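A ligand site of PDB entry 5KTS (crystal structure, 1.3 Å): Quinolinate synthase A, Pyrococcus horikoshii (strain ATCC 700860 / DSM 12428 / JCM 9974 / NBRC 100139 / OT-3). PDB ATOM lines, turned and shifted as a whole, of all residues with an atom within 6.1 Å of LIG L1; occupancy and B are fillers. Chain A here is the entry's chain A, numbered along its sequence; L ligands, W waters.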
ATOM      1  N   HIS A  25       5.580   0.981 -14.641  1.00  0.00           N
ATOM      2  CA  HIS A  25       6.472   2.069 -14.298  1.00  0.00           C
ATOM      3  C   HIS A  25       5.966   2.778 -13.038  1.00  0.00           C
ATOM      4  O   HIS A  25       4.784   2.751 -12.702  1.00  0.00           O
ATOM      5  CB  HIS A  25       6.573   3.065 -15.445  1.00  0.00           C
ATOM      6  CG  HIS A  25       7.615   4.098 -15.227  1.00  0.00           C
ATOM      7  ND1 HIS A  25       7.317   5.343 -14.695  1.00  0.00           N
ATOM      8  CD2 HIS A  25       8.957   4.071 -15.391  1.00  0.00           C
ATOM      9  CE1 HIS A  25       8.431   6.041 -14.562  1.00  0.00           C
ATOM     10  NE2 HIS A  25       9.450   5.288 -14.967  1.00  0.00           N
ATOM     11  N   TYR A  27       5.335   5.763 -12.563  1.00  0.00           N
ATOM     12  CA  TYR A  27       4.381   6.844 -12.792  1.00  0.00           C
ATOM     13  C   TYR A  27       2.977   6.332 -13.068  1.00  0.00           C
ATOM     14  O   TYR A  27       2.091   7.127 -13.379  1.00  0.00           O
ATOM     15  CB  TYR A  27       4.820   7.731 -13.971  1.00  0.00           C
ATOM     16  CG  TYR A  27       6.161   8.430 -13.814  1.00  0.00           C
ATOM     17  CD1 TYR A  27       6.761   8.580 -12.565  1.00  0.00           C
ATOM     18  CD2 TYR A  27       6.826   8.944 -14.931  1.00  0.00           C
ATOM     19  CE1 TYR A  27       7.998   9.223 -12.433  1.00  0.00           C
ATOM     20  CE2 TYR A  27       8.058   9.562 -14.818  1.00  0.00           C
ATOM     21  CZ  TYR A  27       8.646   9.706 -13.566  1.00  0.00           C
ATOM     22  OH  TYR A  27       9.867  10.347 -13.485  1.00  0.00           O
ATOM     23  N   VAL A  62       4.744   3.358 -21.110  1.00  0.00           N
ATOM     24  CA  VAL A  62       4.630   3.923 -22.457  1.00  0.00           C
ATOM     25  C   VAL A  62       5.218   3.003 -23.524  1.00  0.00           C
ATOM     26  O   VAL A  62       5.943   2.039 -23.226  1.00  0.00           O
ATOM     27  CB  VAL A  62       5.211   5.339 -22.526  1.00  0.00           C
ATOM     28  CG1 VAL A  62       4.398   6.285 -21.628  1.00  0.00           C
ATOM     29  CG2 VAL A  62       6.656   5.337 -22.108  1.00  0.00           C
ATOM     30  N   PHE A  64       7.611   3.035 -25.821  1.00  0.00           N
ATOM     31  CA  PHE A  64       9.046   2.755 -25.914  1.00  0.00           C
ATOM     32  C   PHE A  64       9.470   1.723 -24.866  1.00  0.00           C
ATOM     33  O   PHE A  64      10.328   0.877 -25.120  1.00  0.00           O
ATOM     34  CB  PHE A  64       9.915   4.023 -25.910  1.00  0.00           C
ATOM     35  CG  PHE A  64      10.167   4.654 -24.537  1.00  0.00           C
ATOM     36  CD1 PHE A  64      11.065   4.084 -23.643  1.00  0.00           C
ATOM     37  CD2 PHE A  64       9.537   5.836 -24.180  1.00  0.00           C
ATOM     38  CE1 PHE A  64      11.290   4.664 -22.407  1.00  0.00           C
ATOM     39  CE2 PHE A  64       9.791   6.424 -22.941  1.00  0.00           C
ATOM     40  CZ  PHE A  64      10.646   5.836 -22.064  1.00  0.00           C
ATOM     41  N   MET A  65       8.849   1.779 -23.683  1.00  0.00           N
ATOM     42  CA  MET A  65       9.183   0.818 -22.628  1.00  0.00           C
ATOM     43  C   MET A  65       8.711  -0.576 -23.000  1.00  0.00           C
ATOM     44  O   MET A  65       9.449  -1.552 -22.813  1.00  0.00           O
ATOM     45  CB  MET A  65       8.530   1.239 -21.315  1.00  0.00           C
ATOM     46  CG  MET A  65       9.046   2.544 -20.796  1.00  0.00           C
ATOM     47  SD  MET A  65       8.190   3.029 -19.297  1.00  0.00           S
ATOM     48  CE  MET A  65       9.109   4.552 -18.968  1.00  0.00           C
ATOM     49  N   THR A  86       2.349   7.063 -24.892  1.00  0.00           N
ATOM     50  CA  THR A  86       3.601   7.363 -25.578  1.00  0.00           C
ATOM     51  C   THR A  86       4.315   8.519 -24.892  1.00  0.00           C
ATOM     52  O   THR A  86       3.724   9.252 -24.087  1.00  0.00           O
ATOM     53  CB  THR A  86       3.402   7.629 -27.080  1.00  0.00           C
ATOM     54  OG1 THR A  86       4.686   7.656 -27.735  1.00  0.00           O
ATOM     55  CG2 THR A  86       2.694   8.958 -27.299  1.00  0.00           C
ATOM     56  N   CYS A  87       5.591   8.656 -25.224  1.00  0.00           N
ATOM     57  CA  CYS A  87       6.509   9.569 -24.554  1.00  0.00           C
ATOM     58  C   CYS A  87       6.847  10.733 -25.483  1.00  0.00           C
ATOM     59  O   CYS A  87       7.462  10.525 -26.541  1.00  0.00           O
ATOM     60  CB  CYS A  87       7.788   8.840 -24.138  1.00  0.00           C
ATOM     61  SG  CYS A  87       9.098   9.874 -23.466  1.00  0.00           S
ATOM     62  N   ALA A  88       6.488  11.938 -25.051  1.00  0.00           N
ATOM     63  CA  ALA A  88       6.750  13.129 -25.856  1.00  0.00           C
ATOM     64  C   ALA A  88       8.252  13.354 -26.020  1.00  0.00           C
ATOM     65  O   ALA A  88       8.703  13.719 -27.108  1.00  0.00           O
ATOM     66  CB  ALA A  88       6.079  14.345 -25.237  1.00  0.00           C
ATOM     67  N   MET A  89       9.039  13.138 -24.965  1.00  0.00           N
ATOM     68  CA  MET A  89      10.483  13.365 -25.073  1.00  0.00           C
ATOM     69  C   MET A  89      11.113  12.394 -26.064  1.00  0.00           C
ATOM     70  O   MET A  89      11.902  12.803 -26.921  1.00  0.00           O
ATOM     71  CB  MET A  89      11.140  13.273 -23.688  1.00  0.00           C
ATOM     72  CG  MET A  89      12.671  13.528 -23.678  1.00  0.00           C
ATOM     73  SD  MET A  89      13.537  11.944 -23.500  1.00  0.00           S
ATOM     74  CE  MET A  89      13.235  11.734 -21.746  1.00  0.00           C
ATOM     75  N   ALA A  90      10.732  11.115 -26.010  1.00  0.00           N
ATOM     76  CA  ALA A  90      11.348  10.108 -26.871  1.00  0.00           C
ATOM     77  C   ALA A  90      11.037  10.364 -28.333  1.00  0.00           C
ATOM     78  O   ALA A  90      11.882  10.124 -29.216  1.00  0.00           O
ATOM     79  CB  ALA A  90      10.850   8.719 -26.467  1.00  0.00           C
ATOM     80  N   TYR A 113      19.328   7.495 -24.641  1.00  0.00           N
ATOM     81  CA  TYR A 113      18.455   7.333 -23.496  1.00  0.00           C
ATOM     82  C   TYR A 113      17.394   6.333 -23.900  1.00  0.00           C
ATOM     83  O   TYR A 113      16.933   6.330 -25.049  1.00  0.00           O
ATOM     84  CB  TYR A 113      17.814   8.696 -23.209  1.00  0.00           C
ATOM     85  CG  TYR A 113      17.228   8.935 -21.836  1.00  0.00           C
ATOM     86  CD1 TYR A 113      17.540   8.122 -20.751  1.00  0.00           C
ATOM     87  CD2 TYR A 113      16.378  10.011 -21.620  1.00  0.00           C
ATOM     88  CE1 TYR A 113      16.985   8.370 -19.499  1.00  0.00           C
ATOM     89  CE2 TYR A 113      15.842  10.262 -20.394  1.00  0.00           C
ATOM     90  CZ  TYR A 113      16.143   9.444 -19.336  1.00  0.00           C
ATOM     91  OH  TYR A 113      15.582   9.723 -18.113  1.00  0.00           O
ATOM     92  N   ASN A 115      14.497   6.368 -23.242  1.00  0.00           N
ATOM     93  CA  ASN A 115      13.375   7.156 -23.744  1.00  0.00           C
ATOM     94  C   ASN A 115      13.650   7.501 -25.202  1.00  0.00           C
ATOM     95  O   ASN A 115      14.013   8.624 -25.557  1.00  0.00           O
ATOM     96  CB  ASN A 115      13.173   8.435 -22.925  1.00  0.00           C
ATOM     97  CG  ASN A 115      12.965   8.153 -21.442  1.00  0.00           C
ATOM     98  OD1 ASN A 115      13.631   7.307 -20.854  1.00  0.00           O
ATOM     99  ND2 ASN A 115      12.041   8.893 -20.824  1.00  0.00           N
ATOM    100  N   ASP A 150      17.304  13.668 -24.176  1.00  0.00           N
ATOM    101  CA  ASP A 150      16.997  14.665 -23.144  1.00  0.00           C
ATOM    102  C   ASP A 150      18.195  15.573 -22.876  1.00  0.00           C
ATOM    103  O   ASP A 150      19.230  15.120 -22.370  1.00  0.00           O
ATOM    104  CB  ASP A 150      16.537  13.973 -21.861  1.00  0.00           C
ATOM    105  CG  ASP A 150      15.935  14.949 -20.885  1.00  0.00           C
ATOM    106  OD1 ASP A 150      14.701  14.926 -20.692  1.00  0.00           O
ATOM    107  OD2 ASP A 150      16.694  15.750 -20.313  1.00  0.00           O
ATOM    108  N   CYS A 174      11.543  16.646 -21.485  1.00  0.00           N
ATOM    109  CA  CYS A 174      10.300  16.111 -20.960  1.00  0.00           C
ATOM    110  C   CYS A 174       9.456  17.251 -20.397  1.00  0.00           C
ATOM    111  O   CYS A 174       9.884  17.923 -19.450  1.00  0.00           O
ATOM    112  CB  CYS A 174      10.614  15.117 -19.845  1.00  0.00           C
ATOM    113  SG  CYS A 174       9.160  14.669 -18.860  1.00  0.00           S
ATOM    114  N   TYR A 175       8.268  17.474 -20.977  1.00  0.00           N
ATOM    115  CA  TYR A 175       7.427  18.588 -20.533  1.00  0.00           C
ATOM    116  C   TYR A 175       7.034  18.452 -19.060  1.00  0.00           C
ATOM    117  O   TYR A 175       6.818  19.457 -18.377  1.00  0.00           O
ATOM    118  CB  TYR A 175       6.179  18.739 -21.413  1.00  0.00           C
ATOM    119  CG  TYR A 175       5.153  17.643 -21.269  1.00  0.00           C
ATOM    120  CD1 TYR A 175       4.073  17.783 -20.405  1.00  0.00           C
ATOM    121  CD2 TYR A 175       5.247  16.464 -21.997  1.00  0.00           C
ATOM    122  CE1 TYR A 175       3.111  16.786 -20.277  1.00  0.00           C
ATOM    123  CE2 TYR A 175       4.293  15.452 -21.873  1.00  0.00           C
ATOM    124  CZ  TYR A 175       3.239  15.623 -20.998  1.00  0.00           C
ATOM    125  OH  TYR A 175       2.281  14.634 -20.866  1.00  0.00           O
ATOM    126  N   VAL A 176       6.904  17.213 -18.563  1.00  0.00           N
ATOM    127  CA  VAL A 176       6.551  17.016 -17.159  1.00  0.00           C
ATOM    128  C   VAL A 176       7.622  17.605 -16.253  1.00  0.00           C
ATOM    129  O   VAL A 176       7.330  18.380 -15.344  1.00  0.00           O
ATOM    130  CB  VAL A 176       6.332  15.528 -16.860  1.00  0.00           C
ATOM    131  CG1 VAL A 176       5.952  15.329 -15.377  1.00  0.00           C
ATOM    132  CG2 VAL A 176       5.252  14.954 -17.761  1.00  0.00           C
ATOM    133  N   HIS A 177       8.891  17.213 -16.486  1.00  0.00           N
ATOM    134  CA  HIS A 177       9.984  17.665 -15.629  1.00  0.00           C
ATOM    135  C   HIS A 177      10.382  19.111 -15.894  1.00  0.00           C
ATOM    136  O   HIS A 177      10.900  19.783 -14.995  1.00  0.00           O
ATOM    137  CB  HIS A 177      11.173  16.731 -15.754  1.00  0.00           C
ATOM    138  CG  HIS A 177      10.927  15.406 -15.116  1.00  0.00           C
ATOM    139  ND1 HIS A 177      10.441  14.322 -15.820  1.00  0.00           N
ATOM    140  CD2 HIS A 177      11.015  15.011 -13.825  1.00  0.00           C
ATOM    141  CE1 HIS A 177      10.291  13.304 -14.982  1.00  0.00           C
ATOM    142  NE2 HIS A 177      10.630  13.695 -13.770  1.00  0.00           N
ATOM    143  N   GLU A 202      15.981  14.946 -15.377  1.00  0.00           N
ATOM    144  CA  GLU A 202      15.238  15.555 -16.483  1.00  0.00           C
ATOM    145  C   GLU A 202      14.761  16.965 -16.146  1.00  0.00           C
ATOM    146  O   GLU A 202      14.288  17.669 -17.048  1.00  0.00           O
ATOM    147  CB  GLU A 202      14.068  14.662 -16.925  1.00  0.00           C
ATOM    148  CG  GLU A 202      14.513  13.344 -17.568  1.00  0.00           C
ATOM    149  CD  GLU A 202      13.364  12.446 -18.000  1.00  0.00           C
ATOM    150  OE1 GLU A 202      12.210  12.930 -18.085  1.00  0.00           O
ATOM    151  OE2 GLU A 202      13.605  11.238 -18.258  1.00  0.00           O
ATOM    152  N   GLU A 235       7.315  13.220 -11.646  1.00  0.00           N
ATOM    153  CA  GLU A 235       5.906  13.016 -11.926  1.00  0.00           C
ATOM    154  C   GLU A 235       5.179  12.599 -10.645  1.00  0.00           C
ATOM    155  O   GLU A 235       5.672  11.797  -9.863  1.00  0.00           O
ATOM    156  CB  GLU A 235       5.773  11.928 -12.991  1.00  0.00           C
ATOM    157  CG  GLU A 235       4.595  12.057 -13.926  1.00  0.00           C
ATOM    158  CD  GLU A 235       3.326  11.405 -13.414  1.00  0.00           C
ATOM    159  OE1 GLU A 235       3.347  10.797 -12.318  1.00  0.00           O
ATOM    160  OE2 GLU A 235       2.305  11.488 -14.118  1.00  0.00           O
ATOM    161  N   CYS A 260       2.152  13.080 -16.407  1.00  0.00           N
ATOM    162  CA  CYS A 260       2.446  12.570 -17.748  1.00  0.00           C
ATOM    163  C   CYS A 260       1.161  12.000 -18.347  1.00  0.00           C
ATOM    164  O   CYS A 260       0.680  10.944 -17.923  1.00  0.00           O
ATOM    165  CB  CYS A 260       3.536  11.509 -17.721  1.00  0.00           C
ATOM    166  SG  CYS A 260       3.830  10.859 -19.390  1.00  0.00           S
ATOM    167  N   ILE A 261       0.630  12.684 -19.364  1.00  0.00           N
ATOM    168  CA  ILE A 261      -0.589  12.232 -20.041  1.00  0.00           C
ATOM    169  C   ILE A 261      -0.390  10.839 -20.641  1.00  0.00           C
ATOM    170  O   ILE A 261      -1.284   9.989 -20.578  1.00  0.00           O
ATOM    171  CB  ILE A 261      -1.033  13.272 -21.083  1.00  0.00           C
ATOM    172  CG1 ILE A 261      -1.426  14.595 -20.409  1.00  0.00           C
ATOM    173  CG2 ILE A 261      -2.196  12.738 -21.949  1.00  0.00           C
ATOM    174  CD1 ILE A 261      -1.724  15.737 -21.368  1.00  0.00           C
ATOM    175  N   GLY A 262       0.785  10.588 -21.230  1.00  0.00           N
ATOM    176  CA  GLY A 262       1.019   9.285 -21.847  1.00  0.00           C
ATOM    177  C   GLY A 262       0.973   8.137 -20.849  1.00  0.00           C
ATOM    178  O   GLY A 262       0.357   7.095 -21.116  1.00  0.00           O
ATOM    179  N   MET A 263       1.607   8.317 -19.690  1.00  0.00           N
ATOM    180  CA  MET A 263       1.547   7.305 -18.648  1.00  0.00           C
ATOM    181  C   MET A 263       0.105   7.033 -18.246  1.00  0.00           C
ATOM    182  O   MET A 263      -0.277   5.872 -18.035  1.00  0.00           O
ATOM    183  CB  MET A 263       2.356   7.766 -17.443  1.00  0.00           C
ATOM    184  CG  MET A 263       3.855   7.598 -17.648  1.00  0.00           C
ATOM    185  SD  MET A 263       4.342   5.870 -17.657  1.00  0.00           S
ATOM    186  CE  MET A 263       6.100   6.012 -17.957  1.00  0.00           C
HETATM  187 FE1  LIG L   1       8.162  10.747 -21.519  1.00  0.00          FE
HETATM  188 FE2  LIG L   1       6.095  11.033 -19.805  1.00  0.00          FE
HETATM  189 FE3  LIG L   1       8.320  12.597 -19.567  1.00  0.00          FE
HETATM  190 FE4  LIG L   1       8.426   9.889 -19.091  1.00  0.00          FE
HETATM  191  S1  LIG L   1       7.253  11.486 -17.904  1.00  0.00           S
HETATM  192  S2  LIG L   1       9.961  11.211 -20.215  1.00  0.00           S
HETATM  193  S3  LIG L   1       6.926   9.099 -20.617  1.00  0.00           S
HETATM  194  S4  LIG L   1       6.858  12.601 -21.322  1.00  0.00           S
HETATM  195  O1  LG2 L   2      11.855   6.347 -13.849  1.00  0.00           O
HETATM  196  C1  LG2 L   2      12.684   7.331 -14.217  1.00  0.00           C
HETATM  197  O2  LG2 L   2      13.528   7.785 -13.460  1.00  0.00           O
HETATM  198  C2  LG2 L   2      12.573   7.843 -15.585  1.00  0.00           C
HETATM  199  C3  LG2 L   2      11.473   8.821 -15.897  1.00  0.00           C
HETATM  200  C4  LG2 L   2      13.429   7.447 -16.542  1.00  0.00           C
HETATM  201  C5  LG2 L   2      14.555   6.513 -16.315  1.00  0.00           C
HETATM  202  O3  LG2 L   2      14.569   5.687 -15.416  1.00  0.00           O
HETATM  203  O4  LG2 L   2      15.605   6.611 -17.123  1.00  0.00           O
HETATM  204  O   HOH W   1       4.098  11.758 -23.094  1.00  0.00           O
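SG of Cys 87 binds FE1 of LIG L1 (2.3 Å).
A ring nitrogen (NE2) of His 25 sits at hydrogen-bond distance from an oxygen (O1) of LG2 L2, at 2.9 Å.
The side-chain sulfur (SG) of Cys 260 is bound to an iron atom (FE2) of LIG L1, at 2.3 Å.
An iron atom (FE3) of LIG L1 is bound by the side-chain sulfur (SG) of Cys 174, 2.3 Å away.
The side-chain hydroxyl (OH) of Tyr 113 sits close to an oxygen (O4) of LG2 L2, at 3.3 Å.
ND2 of Asn 115 sits close to S2 of LIG L1 (3.2 Å).
The backbone NH (N) of Cys 260 sits at hydrogen-bond distance from the side-chain carboxylate (OE2) of Glu 235.
The side-chain carboxylate of Glu 202 sits at hydrogen-bond distance from a ring nitrogen (ND1) of His 177.
N of Met 263 sits close to SG of Cys 260, 3.4 Å away.
SG of Cys 87 sits close to N of Met 89 (3.6 Å).
ND1 of His 177 lies close to SG of Cys 174, at 3.3 Å.
N of Ala 90 sits close to SG of Cys 87, at 3.3 Å.
The side-chain sulfur (SG) of Cys 260 sits close to the backbone NH (N) of Gly 262 (3.6 Å).
OE2 of Glu 202 is in hydrogen-bond range of OH of Tyr 113 (2.5 Å).
S2 of LIG L1 sits close to OE1 of Glu 202 (3.5 Å).
Merely in contact with LIG L1: Met 89, Tyr 27, Ala 88, Tyr 175 and Val 62.
Hydrophobic or aromatic side chains that line LIG L1: Tyr 27, Val 62, Met 89 and Tyr 175.
Ten residues have an atom within 4 Å of LIG L1: Tyr 27, Val 62, Cys 87, Ala 88, Met 89, Asn 115, Cys 174, Tyr 175, Glu 202 and Cys 260.
The nearest printed residue that does not touch LIG L1 is Val 176 (4.01 Å).
Water W1 lies within hydrogen-bond range of O of Thr 86 (2.7 Å), N of Ala 88 (3.1 Å) and S4 of LIG L1 (3.4 Å).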
